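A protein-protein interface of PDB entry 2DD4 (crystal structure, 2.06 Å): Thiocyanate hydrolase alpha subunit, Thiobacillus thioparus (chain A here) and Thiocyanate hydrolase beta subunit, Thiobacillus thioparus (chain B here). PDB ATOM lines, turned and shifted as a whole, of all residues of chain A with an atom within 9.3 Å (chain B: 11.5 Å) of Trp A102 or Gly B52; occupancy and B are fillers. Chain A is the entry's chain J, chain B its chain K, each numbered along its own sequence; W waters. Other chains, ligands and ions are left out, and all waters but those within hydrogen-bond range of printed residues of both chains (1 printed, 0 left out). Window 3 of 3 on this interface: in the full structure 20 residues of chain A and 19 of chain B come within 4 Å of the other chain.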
ATOM      1  N   MET A  57     -19.743  25.890  20.175  1.00  0.00           N
ATOM      2  CA  MET A  57     -19.613  27.100  20.980  1.00  0.00           C
ATOM      3  C   MET A  57     -18.678  28.162  20.431  1.00  0.00           C
ATOM      4  O   MET A  57     -17.627  27.862  19.861  1.00  0.00           O
ATOM      5  CB  MET A  57     -19.187  26.749  22.409  1.00  0.00           C
ATOM      6  CG  MET A  57     -20.153  25.837  23.167  1.00  0.00           C
ATOM      7  SD  MET A  57     -20.148  24.133  22.578  1.00  0.00           S
ATOM      8  CE  MET A  57     -18.433  23.647  22.991  1.00  0.00           C
ATOM      9  N   THR A  58     -19.069  29.417  20.626  1.00  0.00           N
ATOM     10  CA  THR A  58     -18.276  30.542  20.167  1.00  0.00           C
ATOM     11  C   THR A  58     -16.884  30.525  20.794  1.00  0.00           C
ATOM     12  O   THR A  58     -15.905  30.886  20.146  1.00  0.00           O
ATOM     13  CB  THR A  58     -18.964  31.884  20.520  1.00  0.00           C
ATOM     14  OG1 THR A  58     -20.189  32.006  19.783  1.00  0.00           O
ATOM     15  CG2 THR A  58     -18.048  33.059  20.191  1.00  0.00           C
ATOM     16  N   TYR A  59     -16.783  30.084  22.046  1.00  0.00           N
ATOM     17  CA  TYR A  59     -15.486  30.074  22.710  1.00  0.00           C
ATOM     18  C   TYR A  59     -14.440  29.152  22.085  1.00  0.00           C
ATOM     19  O   TYR A  59     -13.264  29.223  22.441  1.00  0.00           O
ATOM     20  CB  TYR A  59     -15.647  29.772  24.218  1.00  0.00           C
ATOM     21  CG  TYR A  59     -15.952  28.334  24.615  1.00  0.00           C
ATOM     22  CD1 TYR A  59     -14.960  27.352  24.593  1.00  0.00           C
ATOM     23  CD2 TYR A  59     -17.219  27.975  25.085  1.00  0.00           C
ATOM     24  CE1 TYR A  59     -15.216  26.045  25.039  1.00  0.00           C
ATOM     25  CE2 TYR A  59     -17.489  26.676  25.531  1.00  0.00           C
ATOM     26  CZ  TYR A  59     -16.482  25.717  25.508  1.00  0.00           C
ATOM     27  OH  TYR A  59     -16.740  24.442  25.975  1.00  0.00           O
ATOM     28  N   THR A  60     -14.854  28.305  21.142  1.00  0.00           N
ATOM     29  CA  THR A  60     -13.922  27.389  20.485  1.00  0.00           C
ATOM     30  C   THR A  60     -13.449  27.856  19.108  1.00  0.00           C
ATOM     31  O   THR A  60     -12.483  27.316  18.574  1.00  0.00           O
ATOM     32  CB  THR A  60     -14.537  25.988  20.261  1.00  0.00           C
ATOM     33  OG1 THR A  60     -15.641  26.097  19.351  1.00  0.00           O
ATOM     34  CG2 THR A  60     -15.008  25.376  21.576  1.00  0.00           C
ATOM     35  N   ARG A  61     -14.123  28.849  18.535  1.00  0.00           N
ATOM     36  CA  ARG A  61     -13.777  29.320  17.194  1.00  0.00           C
ATOM     37  C   ARG A  61     -12.346  29.805  17.022  1.00  0.00           C
ATOM     38  O   ARG A  61     -11.879  30.675  17.753  1.00  0.00           O
ATOM     39  CB  ARG A  61     -14.747  30.425  16.750  1.00  0.00           C
ATOM     40  CG  ARG A  61     -16.236  30.080  16.901  1.00  0.00           C
ATOM     41  CD  ARG A  61     -16.559  28.685  16.379  1.00  0.00           C
ATOM     42  NE  ARG A  61     -17.991  28.380  16.412  1.00  0.00           N
ATOM     43  CZ  ARG A  61     -18.843  28.682  15.435  1.00  0.00           C
ATOM     44  NH1 ARG A  61     -18.407  29.303  14.345  1.00  0.00           N
ATOM     45  NH2 ARG A  61     -20.126  28.345  15.534  1.00  0.00           N
ATOM     46  N   ALA A  63      -9.706  28.193  17.624  1.00  0.00           N
ATOM     47  CA  ALA A  63      -8.780  27.527  18.528  1.00  0.00           C
ATOM     48  C   ALA A  63      -8.339  26.189  17.939  1.00  0.00           C
ATOM     49  O   ALA A  63      -9.043  25.597  17.117  1.00  0.00           O
ATOM     50  CB  ALA A  63      -9.436  27.310  19.891  1.00  0.00           C
ATOM     51  N   PHE A  96      -8.776  20.659  24.157  1.00  0.00           N
ATOM     52  CA  PHE A  96      -8.127  21.960  24.040  1.00  0.00           C
ATOM     53  C   PHE A  96      -7.356  22.276  25.313  1.00  0.00           C
ATOM     54  O   PHE A  96      -7.795  21.934  26.415  1.00  0.00           O
ATOM     55  CB  PHE A  96      -9.172  23.066  23.862  1.00  0.00           C
ATOM     56  CG  PHE A  96      -9.981  22.961  22.599  1.00  0.00           C
ATOM     57  CD1 PHE A  96      -9.491  23.468  21.397  1.00  0.00           C
ATOM     58  CD2 PHE A  96     -11.257  22.402  22.621  1.00  0.00           C
ATOM     59  CE1 PHE A  96     -10.263  23.424  20.235  1.00  0.00           C
ATOM     60  CE2 PHE A  96     -12.036  22.353  21.468  1.00  0.00           C
ATOM     61  CZ  PHE A  96     -11.538  22.867  20.271  1.00  0.00           C
ATOM     62  N   ALA A  97      -6.209  22.930  25.167  1.00  0.00           N
ATOM     63  CA  ALA A  97      -5.436  23.340  26.332  1.00  0.00           C
ATOM     64  C   ALA A  97      -6.174  24.606  26.778  1.00  0.00           C
ATOM     65  O   ALA A  97      -6.514  25.445  25.945  1.00  0.00           O
ATOM     66  CB  ALA A  97      -4.005  23.669  25.929  1.00  0.00           C
ATOM     67  N   GLN A  98      -6.446  24.744  28.073  1.00  0.00           N
ATOM     68  CA  GLN A  98      -7.170  25.918  28.560  1.00  0.00           C
ATOM     69  C   GLN A  98      -6.509  27.241  28.162  1.00  0.00           C
ATOM     70  O   GLN A  98      -7.197  28.213  27.847  1.00  0.00           O
ATOM     71  CB  GLN A  98      -7.341  25.846  30.081  1.00  0.00           C
ATOM     72  CG  GLN A  98      -8.366  24.810  30.540  1.00  0.00           C
ATOM     73  CD  GLN A  98      -9.803  25.247  30.285  1.00  0.00           C
ATOM     74  OE1 GLN A  98     -10.154  25.669  29.180  1.00  0.00           O
ATOM     75  NE2 GLN A  98     -10.643  25.141  31.309  1.00  0.00           N
ATOM     76  N   LYS A  99      -5.179  27.274  28.160  1.00  0.00           N
ATOM     77  CA  LYS A  99      -4.465  28.493  27.793  1.00  0.00           C
ATOM     78  C   LYS A  99      -4.721  28.902  26.342  1.00  0.00           C
ATOM     79  O   LYS A  99      -4.523  30.060  25.981  1.00  0.00           O
ATOM     80  CB  LYS A  99      -2.963  28.323  28.024  1.00  0.00           C
ATOM     81  CG  LYS A  99      -2.295  27.340  27.073  1.00  0.00           C
ATOM     82  CD  LYS A  99      -0.896  26.967  27.555  1.00  0.00           C
ATOM     83  CE  LYS A  99      -0.008  28.193  27.738  1.00  0.00           C
ATOM     84  NZ  LYS A  99       1.331  27.837  28.298  1.00  0.00           N
ATOM     85  N   ASP A 100      -5.157  27.965  25.506  1.00  0.00           N
ATOM     86  CA  ASP A 100      -5.426  28.299  24.109  1.00  0.00           C
ATOM     87  C   ASP A 100      -6.828  28.856  23.913  1.00  0.00           C
ATOM     88  O   ASP A 100      -7.175  29.337  22.832  1.00  0.00           O
ATOM     89  CB  ASP A 100      -5.224  27.079  23.207  1.00  0.00           C
ATOM     90  CG  ASP A 100      -3.764  26.683  23.089  1.00  0.00           C
ATOM     91  OD1 ASP A 100      -2.907  27.587  23.118  1.00  0.00           O
ATOM     92  OD2 ASP A 100      -3.476  25.478  22.958  1.00  0.00           O
ATOM     93  N   LEU A 101      -7.638  28.790  24.962  1.00  0.00           N
ATOM     94  CA  LEU A 101      -8.994  29.310  24.892  1.00  0.00           C
ATOM     95  C   LEU A 101      -9.094  30.643  25.627  1.00  0.00           C
ATOM     96  O   LEU A 101      -9.644  31.617  25.103  1.00  0.00           O
ATOM     97  CB  LEU A 101      -9.984  28.317  25.506  1.00  0.00           C
ATOM     98  CG  LEU A 101     -10.108  26.949  24.826  1.00  0.00           C
ATOM     99  CD1 LEU A 101     -11.043  26.060  25.639  1.00  0.00           C
ATOM    100  CD2 LEU A 101     -10.637  27.124  23.401  1.00  0.00           C
ATOM    101  N   TRP A 102      -8.539  30.681  26.835  1.00  0.00           N
ATOM    102  CA  TRP A 102      -8.593  31.869  27.677  1.00  0.00           C
ATOM    103  C   TRP A 102      -7.214  32.504  27.865  1.00  0.00           C
ATOM    104  O   TRP A 102      -6.335  31.924  28.500  1.00  0.00           O
ATOM    105  CB  TRP A 102      -9.187  31.483  29.031  1.00  0.00           C
ATOM    106  CG  TRP A 102     -10.197  30.376  28.927  1.00  0.00           C
ATOM    107  CD1 TRP A 102     -10.057  29.089  29.371  1.00  0.00           C
ATOM    108  CD2 TRP A 102     -11.493  30.451  28.317  1.00  0.00           C
ATOM    109  NE1 TRP A 102     -11.187  28.359  29.076  1.00  0.00           N
ATOM    110  CE2 TRP A 102     -12.085  29.172  28.430  1.00  0.00           C
ATOM    111  CE3 TRP A 102     -12.212  31.477  27.685  1.00  0.00           C
ATOM    112  CZ2 TRP A 102     -13.365  28.888  27.935  1.00  0.00           C
ATOM    113  CZ3 TRP A 102     -13.489  31.196  27.191  1.00  0.00           C
ATOM    114  CH2 TRP A 102     -14.049  29.911  27.320  1.00  0.00           C
ATOM    115  N   PRO A 103      -7.016  33.718  27.322  1.00  0.00           N
ATOM    116  CA  PRO A 103      -5.743  34.441  27.420  1.00  0.00           C
ATOM    117  C   PRO A 103      -5.214  34.606  28.842  1.00  0.00           C
ATOM    118  O   PRO A 103      -4.004  34.627  29.054  1.00  0.00           O
ATOM    119  CB  PRO A 103      -6.060  35.789  26.771  1.00  0.00           C
ATOM    120  CG  PRO A 103      -7.122  35.438  25.773  1.00  0.00           C
ATOM    121  CD  PRO A 103      -8.005  34.511  26.572  1.00  0.00           C
ATOM    122  N   GLU A 104      -6.120  34.712  29.811  1.00  0.00           N
ATOM    123  CA  GLU A 104      -5.726  34.906  31.203  1.00  0.00           C
ATOM    124  C   GLU A 104      -5.406  33.635  31.991  1.00  0.00           C
ATOM    125  O   GLU A 104      -4.941  33.721  33.133  1.00  0.00           O
ATOM    126  CB  GLU A 104      -6.812  35.688  31.957  1.00  0.00           C
ATOM    127  CG  GLU A 104      -8.027  34.861  32.408  1.00  0.00           C
ATOM    128  CD  GLU A 104      -8.968  34.476  31.272  1.00  0.00           C
ATOM    129  OE1 GLU A 104      -8.722  34.879  30.114  1.00  0.00           O
ATOM    130  OE2 GLU A 104      -9.963  33.770  31.543  1.00  0.00           O
ATOM    131  N   TYR A 105      -5.646  32.463  31.406  1.00  0.00           N
ATOM    132  CA  TYR A 105      -5.383  31.225  32.134  1.00  0.00           C
ATOM    133  C   TYR A 105      -3.956  31.208  32.668  1.00  0.00           C
ATOM    134  O   TYR A 105      -3.007  31.519  31.952  1.00  0.00           O
ATOM    135  CB  TYR A 105      -5.632  29.992  31.258  1.00  0.00           C
ATOM    136  CG  TYR A 105      -6.272  28.865  32.041  1.00  0.00           C
ATOM    137  CD1 TYR A 105      -7.622  28.922  32.390  1.00  0.00           C
ATOM    138  CD2 TYR A 105      -5.519  27.778  32.493  1.00  0.00           C
ATOM    139  CE1 TYR A 105      -8.212  27.930  33.170  1.00  0.00           C
ATOM    140  CE2 TYR A 105      -6.101  26.777  33.282  1.00  0.00           C
ATOM    141  CZ  TYR A 105      -7.450  26.864  33.615  1.00  0.00           C
ATOM    142  OH  TYR A 105      -8.038  25.895  34.398  1.00  0.00           O
ATOM    143  N   SER A 106      -3.815  30.836  33.934  1.00  0.00           N
ATOM    144  CA  SER A 106      -2.517  30.808  34.598  1.00  0.00           C
ATOM    145  C   SER A 106      -1.604  29.644  34.228  1.00  0.00           C
ATOM    146  O   SER A 106      -2.047  28.501  34.123  1.00  0.00           O
ATOM    147  CB  SER A 106      -2.723  30.820  36.114  1.00  0.00           C
ATOM    148  OG  SER A 106      -1.498  30.609  36.797  1.00  0.00           O
ATOM    149  N   ASP A 107      -0.321  29.944  34.045  1.00  0.00           N
ATOM    150  CA  ASP A 107       0.657  28.915  33.720  1.00  0.00           C
ATOM    151  C   ASP A 107       0.811  27.972  34.908  1.00  0.00           C
ATOM    152  O   ASP A 107       1.360  26.883  34.771  1.00  0.00           O
ATOM    153  CB  ASP A 107       2.022  29.527  33.394  1.00  0.00           C
ATOM    154  CG  ASP A 107       2.018  30.310  32.102  1.00  0.00           C
ATOM    155  OD1 ASP A 107       1.226  29.971  31.196  1.00  0.00           O
ATOM    156  OD2 ASP A 107       2.825  31.256  31.987  1.00  0.00           O
ATOM    157  N   PHE A 109      -1.480  26.422  36.288  1.00  0.00           N
ATOM    158  CA  PHE A 109      -2.348  25.288  35.987  1.00  0.00           C
ATOM    159  C   PHE A 109      -2.160  24.937  34.511  1.00  0.00           C
ATOM    160  O   PHE A 109      -3.118  24.837  33.742  1.00  0.00           O
ATOM    161  CB  PHE A 109      -3.796  25.675  36.283  1.00  0.00           C
ATOM    162  CG  PHE A 109      -3.995  26.240  37.665  1.00  0.00           C
ATOM    163  CD1 PHE A 109      -3.732  25.464  38.792  1.00  0.00           C
ATOM    164  CD2 PHE A 109      -4.429  27.549  37.840  1.00  0.00           C
ATOM    165  CE1 PHE A 109      -3.899  25.988  40.075  1.00  0.00           C
ATOM    166  CE2 PHE A 109      -4.600  28.083  39.119  1.00  0.00           C
ATOM    167  CZ  PHE A 109      -4.333  27.301  40.237  1.00  0.00           C
ATOM    168  N   ASP A 112      -4.318  21.972  32.583  1.00  0.00           N
ATOM    169  CA  ASP A 112      -5.772  21.977  32.483  1.00  0.00           C
ATOM    170  C   ASP A 112      -6.244  21.972  31.033  1.00  0.00           C
ATOM    171  O   ASP A 112      -5.640  22.602  30.163  1.00  0.00           O
ATOM    172  CB  ASP A 112      -6.353  23.180  33.229  1.00  0.00           C
ATOM    173  CG  ASP A 112      -6.206  23.053  34.734  1.00  0.00           C
ATOM    174  OD1 ASP A 112      -5.674  22.021  35.202  1.00  0.00           O
ATOM    175  OD2 ASP A 112      -6.625  23.981  35.452  1.00  0.00           O
ATOM    176  N   THR A 113      -7.339  21.262  30.784  1.00  0.00           N
ATOM    177  CA  THR A 113      -7.873  21.144  29.436  1.00  0.00           C
ATOM    178  C   THR A 113      -9.394  21.197  29.402  1.00  0.00           C
ATOM    179  O   THR A 113     -10.056  21.234  30.442  1.00  0.00           O
ATOM    180  CB  THR A 113      -7.448  19.812  28.806  1.00  0.00           C
ATOM    181  OG1 THR A 113      -7.901  18.744  29.645  1.00  0.00           O
ATOM    182  CG2 THR A 113      -5.925  19.730  28.668  1.00  0.00           C
ATOM    183  N   LEU A 114      -9.933  21.198  28.188  1.00  0.00           N
ATOM    184  CA  LEU A 114     -11.373  21.221  27.965  1.00  0.00           C
ATOM    185  C   LEU A 114     -11.660  20.265  26.808  1.00  0.00           C
ATOM    186  O   LEU A 114     -11.022  20.352  25.758  1.00  0.00           O
ATOM    187  CB  LEU A 114     -11.838  22.644  27.617  1.00  0.00           C
ATOM    188  CG  LEU A 114     -13.343  22.865  27.400  1.00  0.00           C
ATOM    189  CD1 LEU A 114     -13.700  24.303  27.734  1.00  0.00           C
ATOM    190  CD2 LEU A 114     -13.729  22.534  25.961  1.00  0.00           C
ATOM    191  N   ARG B  45     -26.537  36.395  17.519  1.00  0.00           N
ATOM    192  CA  ARG B  45     -25.964  35.274  18.265  1.00  0.00           C
ATOM    193  C   ARG B  45     -27.055  34.240  18.523  1.00  0.00           C
ATOM    194  O   ARG B  45     -28.248  34.526  18.391  1.00  0.00           O
ATOM    195  CB  ARG B  45     -25.474  35.748  19.640  1.00  0.00           C
ATOM    196  CG  ARG B  45     -26.661  36.083  20.567  1.00  0.00           C
ATOM    197  CD  ARG B  45     -26.281  36.445  22.000  1.00  0.00           C
ATOM    198  NE  ARG B  45     -25.518  35.392  22.659  1.00  0.00           N
ATOM    199  CZ  ARG B  45     -25.269  35.354  23.963  1.00  0.00           C
ATOM    200  NH1 ARG B  45     -25.733  36.309  24.762  1.00  0.00           N
ATOM    201  NH2 ARG B  45     -24.537  34.371  24.469  1.00  0.00           N
ATOM    202  N   VAL B  46     -26.634  33.043  18.911  1.00  0.00           N
ATOM    203  CA  VAL B  46     -27.563  31.982  19.268  1.00  0.00           C
ATOM    204  C   VAL B  46     -27.559  32.113  20.797  1.00  0.00           C
ATOM    205  O   VAL B  46     -26.555  31.834  21.446  1.00  0.00           O
ATOM    206  CB  VAL B  46     -27.020  30.604  18.832  1.00  0.00           C
ATOM    207  CG1 VAL B  46     -28.109  29.573  18.922  1.00  0.00           C
ATOM    208  CG2 VAL B  46     -26.491  30.679  17.399  1.00  0.00           C
ATOM    209  N   PRO B  47     -28.682  32.562  21.384  1.00  0.00           N
ATOM    210  CA  PRO B  47     -28.868  32.770  22.827  1.00  0.00           C
ATOM    211  C   PRO B  47     -28.307  31.740  23.814  1.00  0.00           C
ATOM    212  O   PRO B  47     -27.838  32.111  24.888  1.00  0.00           O
ATOM    213  CB  PRO B  47     -30.384  32.915  22.959  1.00  0.00           C
ATOM    214  CG  PRO B  47     -30.757  33.578  21.671  1.00  0.00           C
ATOM    215  CD  PRO B  47     -29.949  32.792  20.665  1.00  0.00           C
ATOM    216  N   HIS B  48     -28.347  30.458  23.460  1.00  0.00           N
ATOM    217  CA  HIS B  48     -27.874  29.419  24.370  1.00  0.00           C
ATOM    218  C   HIS B  48     -26.356  29.296  24.526  1.00  0.00           C
ATOM    219  O   HIS B  48     -25.876  28.656  25.462  1.00  0.00           O
ATOM    220  CB  HIS B  48     -28.464  28.057  23.964  1.00  0.00           C
ATOM    221  CG  HIS B  48     -27.927  27.510  22.675  1.00  0.00           C
ATOM    222  ND1 HIS B  48     -28.238  26.246  22.223  1.00  0.00           N
ATOM    223  CD2 HIS B  48     -27.094  28.045  21.750  1.00  0.00           C
ATOM    224  CE1 HIS B  48     -27.616  26.022  21.077  1.00  0.00           C
ATOM    225  NE2 HIS B  48     -26.915  27.099  20.768  1.00  0.00           N
ATOM    226  N   ASP B  49     -25.610  29.921  23.621  1.00  0.00           N
ATOM    227  CA  ASP B  49     -24.147  29.859  23.625  1.00  0.00           C
ATOM    228  C   ASP B  49     -23.530  30.864  24.607  1.00  0.00           C
ATOM    229  O   ASP B  49     -23.025  31.908  24.194  1.00  0.00           O
ATOM    230  CB  ASP B  49     -23.658  30.121  22.192  1.00  0.00           C
ATOM    231  CG  ASP B  49     -22.182  29.859  22.015  1.00  0.00           C
ATOM    232  OD1 ASP B  49     -21.550  29.306  22.941  1.00  0.00           O
ATOM    233  OD2 ASP B  49     -21.657  30.202  20.934  1.00  0.00           O
ATOM    234  N   VAL B  50     -23.551  30.534  25.899  1.00  0.00           N
ATOM    235  CA  VAL B  50     -23.042  31.434  26.934  1.00  0.00           C
ATOM    236  C   VAL B  50     -21.688  31.086  27.559  1.00  0.00           C
ATOM    237  O   VAL B  50     -21.169  31.853  28.366  1.00  0.00           O
ATOM    238  CB  VAL B  50     -24.066  31.572  28.093  1.00  0.00           C
ATOM    239  CG1 VAL B  50     -25.438  31.927  27.530  1.00  0.00           C
ATOM    240  CG2 VAL B  50     -24.140  30.269  28.895  1.00  0.00           C
ATOM    241  N   GLY B  51     -21.115  29.941  27.197  1.00  0.00           N
ATOM    242  CA  GLY B  51     -19.837  29.552  27.771  1.00  0.00           C
ATOM    243  C   GLY B  51     -18.730  30.583  27.620  1.00  0.00           C
ATOM    244  O   GLY B  51     -18.492  31.097  26.529  1.00  0.00           O
ATOM    245  N   GLY B  52     -18.042  30.884  28.720  1.00  0.00           N
ATOM    246  CA  GLY B  52     -16.958  31.851  28.660  1.00  0.00           C
ATOM    247  C   GLY B  52     -17.358  33.252  29.084  1.00  0.00           C
ATOM    248  O   GLY B  52     -16.498  34.080  29.375  1.00  0.00           O
ATOM    249  N   GLU B  53     -18.660  33.527  29.108  1.00  0.00           N
ATOM    250  CA  GLU B  53     -19.148  34.841  29.517  1.00  0.00           C
ATOM    251  C   GLU B  53     -18.847  35.061  30.994  1.00  0.00           C
ATOM    252  O   GLU B  53     -19.023  34.162  31.813  1.00  0.00           O
ATOM    253  CB  GLU B  53     -20.657  34.950  29.276  1.00  0.00           C
ATOM    254  CG  GLU B  53     -21.040  35.155  27.822  1.00  0.00           C
ATOM    255  CD  GLU B  53     -22.542  35.111  27.603  1.00  0.00           C
ATOM    256  OE1 GLU B  53     -23.298  35.401  28.557  1.00  0.00           O
ATOM    257  OE2 GLU B  53     -22.965  34.801  26.472  1.00  0.00           O
ATOM    258  N   ALA B  54     -18.384  36.258  31.330  1.00  0.00           N
ATOM    259  CA  ALA B  54     -18.067  36.577  32.712  1.00  0.00           C
ATOM    260  C   ALA B  54     -19.348  36.623  33.538  1.00  0.00           C
ATOM    261  O   ALA B  54     -20.365  37.157  33.098  1.00  0.00           O
ATOM    262  CB  ALA B  54     -17.344  37.918  32.786  1.00  0.00           C
ATOM    263  N   ASP B  55     -19.306  36.034  34.724  1.00  0.00           N
ATOM    264  CA  ASP B  55     -20.461  36.049  35.614  1.00  0.00           C
ATOM    265  C   ASP B  55     -19.891  36.059  37.022  1.00  0.00           C
ATOM    266  O   ASP B  55     -18.693  35.845  37.207  1.00  0.00           O
ATOM    267  CB  ASP B  55     -21.344  34.811  35.405  1.00  0.00           C
ATOM    268  CG  ASP B  55     -22.781  35.030  35.874  1.00  0.00           C
ATOM    269  OD1 ASP B  55     -23.004  35.883  36.758  1.00  0.00           O
ATOM    270  OD2 ASP B  55     -23.690  34.340  35.366  1.00  0.00           O
ATOM    271  N   VAL B  56     -20.743  36.302  38.011  1.00  0.00           N
ATOM    272  CA  VAL B  56     -20.296  36.367  39.394  1.00  0.00           C
ATOM    273  C   VAL B  56     -20.475  35.052  40.142  1.00  0.00           C
ATOM    274  O   VAL B  56     -21.077  34.105  39.635  1.00  0.00           O
ATOM    275  CB  VAL B  56     -21.074  37.456  40.169  1.00  0.00           C
ATOM    276  CG1 VAL B  56     -20.998  38.780  39.425  1.00  0.00           C
ATOM    277  CG2 VAL B  56     -22.522  37.027  40.360  1.00  0.00           C
ATOM    278  N   TYR B  60     -24.873  28.357  44.892  1.00  0.00           N
ATOM    279  CA  TYR B  60     -25.744  27.438  44.169  1.00  0.00           C
ATOM    280  C   TYR B  60     -26.757  26.751  45.067  1.00  0.00           C
ATOM    281  O   TYR B  60     -26.429  26.285  46.158  1.00  0.00           O
ATOM    282  CB  TYR B  60     -24.910  26.381  43.439  1.00  0.00           C
ATOM    283  CG  TYR B  60     -24.076  26.935  42.304  1.00  0.00           C
ATOM    284  CD1 TYR B  60     -24.678  27.594  41.228  1.00  0.00           C
ATOM    285  CD2 TYR B  60     -22.687  26.802  42.302  1.00  0.00           C
ATOM    286  CE1 TYR B  60     -23.914  28.104  40.179  1.00  0.00           C
ATOM    287  CE2 TYR B  60     -21.913  27.313  41.254  1.00  0.00           C
ATOM    288  CZ  TYR B  60     -22.536  27.964  40.197  1.00  0.00           C
ATOM    289  OH  TYR B  60     -21.778  28.483  39.164  1.00  0.00           O
HETATM  290  O   HOH W   1     -19.307  30.605  23.781  1.00  0.00           O
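Water W1 lies within hydrogen-bond range of the side-chain carboxylate (OD1) of Asp B49, the backbone carbonyl oxygen (O) of Gly B51, the backbone NH (N) of Tyr A59 and the backbone NH (N) of Thr A58.
Along chain B the printed residues that touch a printed residue of chain A span positions 49 to 52. Of the 22 printed residues of chain A, 4 touch a printed residue of chain B. Printed residues of chain A that touch a printed residue of chain B: Met A57, Thr A58, Tyr A59 and Trp A102. Hydrophobic or aromatic side chains of chain A that line the printed part of chain B: Met A57, Tyr A59 and Trp A102.
Printed residues of chain B within 4 Å of Met A57: Asp B49. Printed residues of chain B within 4 Å of Thr A58: Asp B49. No residue of chain B comes within 4 Å of Leu A101. Of chain B, only Gly B52 (3.7 Å) comes within 4 Å of Trp A102. No residue of chain B comes within 4 Å of Pro A103. No residue of chain B comes within 4 Å of Glu A104. No residue of chain B comes within 4 Å of Tyr A105. Leu A114 touches none of the printed residues of chain B. Of the printed residues of chain A, Asp B49 touches Met A57 (3.5 Å) and Thr A58 (2.6 Å). Printed residues of chain A within 4 Å of Gly B51: Tyr A59. Gly B52 touches just one residue of chain A: Trp A102 (3.7 Å). The nearest residue of chain B that does not touch Trp A102 is Gly B51 (4.7 Å). The nearest printed residue of chain B that does not touch Thr A58 is Gly B51 (6.0 Å).
O of Met A57 is in hydrogen-bond range of OG1 of Thr A60, at 2.7 Å. The backbone carbonyl oxygen (O) of Asp B49 lies within hydrogen-bond range of the guanidinium group (NH2) of Arg B45 (2.9 Å). The side-chain amide oxygen of Gln A98 sits at hydrogen-bond distance from the indole nitrogen of Trp A102 (2.9 Å).
The side-chain hydroxyl (OG1) of Thr A58 sits at hydrogen-bond distance from the side-chain carboxylate (OD2) of Asp B49 (2.6 Å).
Asp B49 touches Met A57 (OD1 to CB, 3.5 Å). Gly B51 touches Tyr A59 (O to CD2, 3.7 Å). Trp A102 touches Gly B52 (CH2 to CA, 3.7 Å).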
